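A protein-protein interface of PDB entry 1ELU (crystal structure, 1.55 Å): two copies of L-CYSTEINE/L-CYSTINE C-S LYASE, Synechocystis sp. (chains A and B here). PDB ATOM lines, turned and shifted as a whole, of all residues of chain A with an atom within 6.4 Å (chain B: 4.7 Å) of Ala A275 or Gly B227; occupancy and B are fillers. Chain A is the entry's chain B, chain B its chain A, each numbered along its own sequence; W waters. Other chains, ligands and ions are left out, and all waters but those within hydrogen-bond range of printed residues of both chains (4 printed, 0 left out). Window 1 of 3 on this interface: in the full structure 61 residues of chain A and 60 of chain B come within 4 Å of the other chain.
The backbone NH of Val B228 is in hydrogen-bond range of the backbone carbonyl oxygen of Asp B83, 3.1 Å away. The backbone NH (N) of Val A228 sits at hydrogen-bond distance from the backbone carbonyl oxygen (O) of Asp A83 (3.1 Å). The side-chain hydroxyl (OG) of Ser A274 lies close to the side-chain hydroxyl (OH) of Tyr A279, 3.3 Å away. The backbone carbonyl oxygen (O) of Ala B275 lies close to the side-chain amide nitrogen (NE2) of Gln B278, 3.1 Å away.
Water W3 lies within hydrogen-bond range of OD1 of Asp B83 and OD1 of Asp A83. Water W4 lies within hydrogen-bond range of the side-chain carboxylate of Asp A83, the side-chain hydroxyl of Ser A274 and the side-chain carboxylate of Asp B83. Water W1 bridges O of Ala B226 (2.8 Å) and OH of Tyr A40 (3.2 Å). Water W2 lies within hydrogen-bond range of N of Ala B275 (3.0 Å) and O of Gly A227 (3.4 Å).
Of the printed residues of chain B, Ala A275 touches Ala B226 and Gly B227. Gly B227 touches three residues of chain A. Of the printed residues of chain B, Tyr A40 touches Gln B278. Printed residues of chain A within 4 Å of Ala B275: Gly A227 (3.8 Å) and Gln A278 (3.0 Å). The nearest printed residue of chain B that does not touch Asp A83 is Ala B275 (6.3 Å).
Printed residues of chain B that touch a printed residue of chain A: Asp B83, Ala B226, Gly B227, Ala B275 and Gln B278. Of the 12 printed residues of chain A, 7 touch a printed residue of chain B. Hydrophobic or aromatic side chains of chain A within 4 Å of the printed part of chain B: Tyr A40 and Ala A275. Among the printed residues, no Asp or Glu carboxylate lies within 4 Å of a Lys or Arg side-chain nitrogen of the other chain.
Ala B275 touches Gly A227 (N to CA, 3.8 Å). Asp B83 touches Thr A273 (O to O, 3.5 Å). CB of Ala B226 touches CG2 of Thr A273 (3.6 Å). CG2 of Thr A273 touches N of Gly B227 (3.8 Å). Ala B226 touches Ser A274. C of Ser A274 touches CA of Gly B227, 3.7 Å away. O of Ala B226 touches CA of Ala A275, at 3.4 Å. N of Ala A275 touches CA of Gly B227, 3.7 Å away. Gln A278 touches Ala B275. Gln A278 touches Gln B278 (OE1 to NE2, 3.5 Å).
Asp B83 touches its own counterpart, Asp A83. Gly A227 touches Ala B275, and with the chains exchanged Ala A275 touches Gly B227. Gln A278 touches Ala B275, but with the chains exchanged Ala A275 does not touch Gln B278 (4.2 Å). Gln A278 touches its own counterpart, Gln B278. Positions printed for both chains: 83, 227, 228, 275 and 278. Of the 12 pairs that touch across the chains among the printed residues, 4 have their exchanged pair printed and touching as well.
The side-chain carboxylate of Asp B83 sits close to the side-chain carboxylate of Asp A83, 2.6 Å away. The side-chain hydroxyl (OH) of Tyr A40 is in hydrogen-bond range of the side-chain amide oxygen (OE1) of Gln B278.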
ATOM      1  N   TYR A  40     -10.317  -5.141  -9.799  1.00  0.00           N
ATOM      2  CA  TYR A  40     -10.667  -4.643  -8.445  1.00  0.00           C
ATOM      3  C   TYR A  40      -9.458  -4.766  -7.571  1.00  0.00           C
ATOM      4  O   TYR A  40      -9.180  -3.884  -6.756  1.00  0.00           O
ATOM      5  CB  TYR A  40     -11.808  -5.435  -7.795  1.00  0.00           C
ATOM      6  CG  TYR A  40     -13.139  -5.000  -8.278  1.00  0.00           C
ATOM      7  CD1 TYR A  40     -13.922  -5.824  -9.095  1.00  0.00           C
ATOM      8  CD2 TYR A  40     -13.630  -3.729  -7.955  1.00  0.00           C
ATOM      9  CE1 TYR A  40     -15.157  -5.386  -9.580  1.00  0.00           C
ATOM     10  CE2 TYR A  40     -14.841  -3.299  -8.425  1.00  0.00           C
ATOM     11  CZ  TYR A  40     -15.602  -4.101  -9.229  1.00  0.00           C
ATOM     12  OH  TYR A  40     -16.797  -3.641  -9.718  1.00  0.00           O
ATOM     13  N   ASP A  83     -22.136   2.378 -22.105  1.00  0.00           N
ATOM     14  CA  ASP A  83     -22.557   1.308 -21.204  1.00  0.00           C
ATOM     15  C   ASP A  83     -23.445   0.273 -21.875  1.00  0.00           C
ATOM     16  O   ASP A  83     -23.597  -0.822 -21.342  1.00  0.00           O
ATOM     17  CB  ASP A  83     -23.400   1.805 -20.049  1.00  0.00           C
ATOM     18  CG  ASP A  83     -22.730   2.840 -19.219  1.00  0.00           C
ATOM     19  OD1 ASP A  83     -23.492   3.625 -18.603  1.00  0.00           O
ATOM     20  OD2 ASP A  83     -21.488   2.878 -19.156  1.00  0.00           O
ATOM     21  N   GLY A 227     -23.179  -3.743 -18.830  1.00  0.00           N
ATOM     22  CA  GLY A 227     -22.627  -2.445 -18.510  1.00  0.00           C
ATOM     23  C   GLY A 227     -21.550  -1.811 -19.368  1.00  0.00           C
ATOM     24  O   GLY A 227     -21.082  -0.724 -19.041  1.00  0.00           O
ATOM     25  N   VAL A 228     -21.133  -2.481 -20.445  1.00  0.00           N
ATOM     26  CA  VAL A 228     -20.118  -1.917 -21.332  1.00  0.00           C
ATOM     27  C   VAL A 228     -20.514  -2.166 -22.793  1.00  0.00           C
ATOM     28  O   VAL A 228     -20.821  -3.312 -23.192  1.00  0.00           O
ATOM     29  CB  VAL A 228     -18.744  -2.545 -21.101  1.00  0.00           C
ATOM     30  CG1 VAL A 228     -17.664  -1.749 -21.854  1.00  0.00           C
ATOM     31  CG2 VAL A 228     -18.433  -2.527 -19.598  1.00  0.00           C
ATOM     32  N   THR A 273     -16.891   8.900 -14.305  1.00  0.00           N
ATOM     33  CA  THR A 273     -16.535   7.586 -13.748  1.00  0.00           C
ATOM     34  C   THR A 273     -17.467   6.477 -14.218  1.00  0.00           C
ATOM     35  O   THR A 273     -18.679   6.635 -14.205  1.00  0.00           O
ATOM     36  CB  THR A 273     -16.537   7.638 -12.197  1.00  0.00           C
ATOM     37  OG1 THR A 273     -15.634   8.658 -11.762  1.00  0.00           O
ATOM     38  CG2 THR A 273     -16.049   6.326 -11.614  1.00  0.00           C
ATOM     39  N   SER A 274     -16.878   5.365 -14.654  1.00  0.00           N
ATOM     40  CA  SER A 274     -17.616   4.185 -15.124  1.00  0.00           C
ATOM     41  C   SER A 274     -17.066   2.964 -14.408  1.00  0.00           C
ATOM     42  O   SER A 274     -16.074   3.063 -13.705  1.00  0.00           O
ATOM     43  CB  SER A 274     -17.409   4.004 -16.634  1.00  0.00           C
ATOM     44  OG  SER A 274     -18.034   5.042 -17.348  1.00  0.00           O
ATOM     45  N   ALA A 275     -17.692   1.814 -14.620  1.00  0.00           N
ATOM     46  CA  ALA A 275     -17.231   0.591 -13.957  1.00  0.00           C
ATOM     47  C   ALA A 275     -16.021   0.006 -14.679  1.00  0.00           C
ATOM     48  O   ALA A 275     -16.133  -0.939 -15.471  1.00  0.00           O
ATOM     49  CB  ALA A 275     -18.374  -0.438 -13.894  1.00  0.00           C
ATOM     50  N   TYR A 276     -14.865   0.571 -14.391  1.00  0.00           N
ATOM     51  CA  TYR A 276     -13.647   0.142 -15.051  1.00  0.00           C
ATOM     52  C   TYR A 276     -13.320  -1.345 -15.026  1.00  0.00           C
ATOM     53  O   TYR A 276     -12.864  -1.882 -16.033  1.00  0.00           O
ATOM     54  CB  TYR A 276     -12.477   0.936 -14.509  1.00  0.00           C
ATOM     55  CG  TYR A 276     -12.740   2.424 -14.499  1.00  0.00           C
ATOM     56  CD1 TYR A 276     -12.547   3.165 -13.336  1.00  0.00           C
ATOM     57  CD2 TYR A 276     -13.153   3.102 -15.650  1.00  0.00           C
ATOM     58  CE1 TYR A 276     -12.751   4.556 -13.315  1.00  0.00           C
ATOM     59  CE2 TYR A 276     -13.369   4.491 -15.649  1.00  0.00           C
ATOM     60  CZ  TYR A 276     -13.161   5.213 -14.471  1.00  0.00           C
ATOM     61  OH  TYR A 276     -13.340   6.588 -14.430  1.00  0.00           O
ATOM     62  N   PRO A 277     -13.520  -2.051 -13.903  1.00  0.00           N
ATOM     63  CA  PRO A 277     -13.194  -3.487 -13.923  1.00  0.00           C
ATOM     64  C   PRO A 277     -13.973  -4.193 -15.038  1.00  0.00           C
ATOM     65  O   PRO A 277     -13.474  -5.139 -15.660  1.00  0.00           O
ATOM     66  CB  PRO A 277     -13.610  -3.957 -12.522  1.00  0.00           C
ATOM     67  CG  PRO A 277     -13.289  -2.731 -11.697  1.00  0.00           C
ATOM     68  CD  PRO A 277     -13.890  -1.610 -12.545  1.00  0.00           C
ATOM     69  N   GLN A 278     -15.191  -3.730 -15.298  1.00  0.00           N
ATOM     70  CA  GLN A 278     -16.010  -4.312 -16.357  1.00  0.00           C
ATOM     71  C   GLN A 278     -15.400  -4.087 -17.734  1.00  0.00           C
ATOM     72  O   GLN A 278     -15.609  -4.908 -18.631  1.00  0.00           O
ATOM     73  CB  GLN A 278     -17.412  -3.755 -16.272  1.00  0.00           C
ATOM     74  CG  GLN A 278     -18.067  -4.220 -14.996  1.00  0.00           C
ATOM     75  CD  GLN A 278     -19.463  -4.525 -15.235  1.00  0.00           C
ATOM     76  OE1 GLN A 278     -19.938  -5.607 -14.910  1.00  0.00           O
ATOM     77  NE2 GLN A 278     -20.161  -3.587 -15.850  1.00  0.00           N
ATOM     78  N   TYR A 279     -14.635  -3.012 -17.894  1.00  0.00           N
ATOM     79  CA  TYR A 279     -13.988  -2.761 -19.190  1.00  0.00           C
ATOM     80  C   TYR A 279     -12.982  -3.886 -19.399  1.00  0.00           C
ATOM     81  O   TYR A 279     -12.839  -4.401 -20.525  1.00  0.00           O
ATOM     82  CB  TYR A 279     -13.253  -1.411 -19.173  1.00  0.00           C
ATOM     83  CG  TYR A 279     -14.119  -0.155 -19.298  1.00  0.00           C
ATOM     84  CD1 TYR A 279     -13.518   1.092 -19.494  1.00  0.00           C
ATOM     85  CD2 TYR A 279     -15.510  -0.192 -19.243  1.00  0.00           C
ATOM     86  CE1 TYR A 279     -14.254   2.253 -19.639  1.00  0.00           C
ATOM     87  CE2 TYR A 279     -16.274   0.994 -19.371  1.00  0.00           C
ATOM     88  CZ  TYR A 279     -15.631   2.220 -19.575  1.00  0.00           C
ATOM     89  OH  TYR A 279     -16.318   3.389 -19.696  1.00  0.00           O
ATOM     90  N   ALA A 280     -12.249  -4.266 -18.348  1.00  0.00           N
ATOM     91  CA  ALA A 280     -11.277  -5.369 -18.461  1.00  0.00           C
ATOM     92  C   ALA A 280     -12.027  -6.673 -18.806  1.00  0.00           C
ATOM     93  O   ALA A 280     -11.501  -7.542 -19.516  1.00  0.00           O
ATOM     94  CB  ALA A 280     -10.472  -5.563 -17.142  1.00  0.00           C
ATOM     95  N   THR B  82     -27.695   6.485 -11.241  1.00  0.00           N
ATOM     96  CA  THR B  82     -26.841   6.878 -12.362  1.00  0.00           C
ATOM     97  C   THR B  82     -25.501   6.132 -12.204  1.00  0.00           C
ATOM     98  O   THR B  82     -25.392   5.198 -11.388  1.00  0.00           O
ATOM     99  CB  THR B  82     -26.527   8.392 -12.306  1.00  0.00           C
ATOM    100  OG1 THR B  82     -25.807   8.650 -11.093  1.00  0.00           O
ATOM    101  CG2 THR B  82     -27.844   9.247 -12.300  1.00  0.00           C
ATOM    102  N   ASP B  83     -24.492   6.540 -12.980  1.00  0.00           N
ATOM    103  CA  ASP B  83     -23.164   5.936 -12.879  1.00  0.00           C
ATOM    104  C   ASP B  83     -22.195   6.806 -12.106  1.00  0.00           C
ATOM    105  O   ASP B  83     -21.161   6.312 -11.703  1.00  0.00           O
ATOM    106  CB  ASP B  83     -22.486   5.726 -14.242  1.00  0.00           C
ATOM    107  CG  ASP B  83     -23.304   4.915 -15.199  1.00  0.00           C
ATOM    108  OD1 ASP B  83     -24.121   4.100 -14.735  1.00  0.00           O
ATOM    109  OD2 ASP B  83     -23.100   5.088 -16.437  1.00  0.00           O
ATOM    110  N   PRO B 225     -18.250   0.922  -5.435  1.00  0.00           N
ATOM    111  CA  PRO B 225     -17.358   0.734  -6.588  1.00  0.00           C
ATOM    112  C   PRO B 225     -17.540   1.848  -7.593  1.00  0.00           C
ATOM    113  O   PRO B 225     -18.605   2.460  -7.655  1.00  0.00           O
ATOM    114  CB  PRO B 225     -17.843  -0.616  -7.151  1.00  0.00           C
ATOM    115  CG  PRO B 225     -19.298  -0.624  -6.869  1.00  0.00           C
ATOM    116  CD  PRO B 225     -19.302  -0.108  -5.413  1.00  0.00           C
ATOM    117  N   ALA B 226     -16.496   2.131  -8.379  1.00  0.00           N
ATOM    118  CA  ALA B 226     -16.616   3.080  -9.474  1.00  0.00           C
ATOM    119  C   ALA B 226     -17.766   2.633 -10.421  1.00  0.00           C
ATOM    120  O   ALA B 226     -17.927   1.440 -10.718  1.00  0.00           O
ATOM    121  CB  ALA B 226     -15.291   3.111 -10.250  1.00  0.00           C
ATOM    122  N   GLY B 227     -18.579   3.592 -10.874  1.00  0.00           N
ATOM    123  CA  GLY B 227     -19.659   3.277 -11.789  1.00  0.00           C
ATOM    124  C   GLY B 227     -21.097   3.333 -11.291  1.00  0.00           C
ATOM    125  O   GLY B 227     -22.025   3.039 -12.046  1.00  0.00           O
ATOM    126  N   VAL B 228     -21.307   3.668 -10.021  1.00  0.00           N
ATOM    127  CA  VAL B 228     -22.684   3.779  -9.534  1.00  0.00           C
ATOM    128  C   VAL B 228     -22.816   5.058  -8.701  1.00  0.00           C
ATOM    129  O   VAL B 228     -21.971   5.335  -7.868  1.00  0.00           O
ATOM    130  CB  VAL B 228     -23.113   2.572  -8.669  1.00  0.00           C
ATOM    131  CG1 VAL B 228     -24.620   2.577  -8.503  1.00  0.00           C
ATOM    132  CG2 VAL B 228     -22.684   1.257  -9.360  1.00  0.00           C
ATOM    133  N   GLY B 229     -23.867   5.822  -8.991  1.00  0.00           N
ATOM    134  CA  GLY B 229     -24.141   7.078  -8.292  1.00  0.00           C
ATOM    135  C   GLY B 229     -25.646   7.321  -8.312  1.00  0.00           C
ATOM    136  O   GLY B 229     -26.437   6.417  -8.612  1.00  0.00           O
ATOM    137  N   ALA B 275     -24.133  -1.892 -15.032  1.00  0.00           N
ATOM    138  CA  ALA B 275     -23.315  -2.841 -14.283  1.00  0.00           C
ATOM    139  C   ALA B 275     -24.044  -3.298 -13.005  1.00  0.00           C
ATOM    140  O   ALA B 275     -23.669  -2.890 -11.906  1.00  0.00           O
ATOM    141  CB  ALA B 275     -21.998  -2.177 -13.905  1.00  0.00           C
ATOM    142  N   GLN B 278     -22.366  -4.170  -9.674  1.00  0.00           N
ATOM    143  CA  GLN B 278     -21.835  -3.011  -8.973  1.00  0.00           C
ATOM    144  C   GLN B 278     -22.931  -2.355  -8.134  1.00  0.00           C
ATOM    145  O   GLN B 278     -22.631  -1.746  -7.121  1.00  0.00           O
ATOM    146  CB  GLN B 278     -21.224  -2.011  -9.976  1.00  0.00           C
ATOM    147  CG  GLN B 278     -19.770  -2.364 -10.424  1.00  0.00           C
ATOM    148  CD  GLN B 278     -19.678  -3.608 -11.281  1.00  0.00           C
ATOM    149  OE1 GLN B 278     -18.614  -4.266 -11.369  1.00  0.00           O
ATOM    150  NE2 GLN B 278     -20.768  -3.932 -11.944  1.00  0.00           N
HETATM  151  O   HOH W   1     -15.965  -0.579 -10.304  1.00  0.00           O
HETATM  152  O   HOH W   2     -22.679   0.410 -16.213  1.00  0.00           O
HETATM  153  O   HOH W   3     -24.741   2.397 -16.518  1.00  0.00           O
HETATM  154  O   HOH W   4     -20.563   4.164 -17.160  1.00  0.00           O
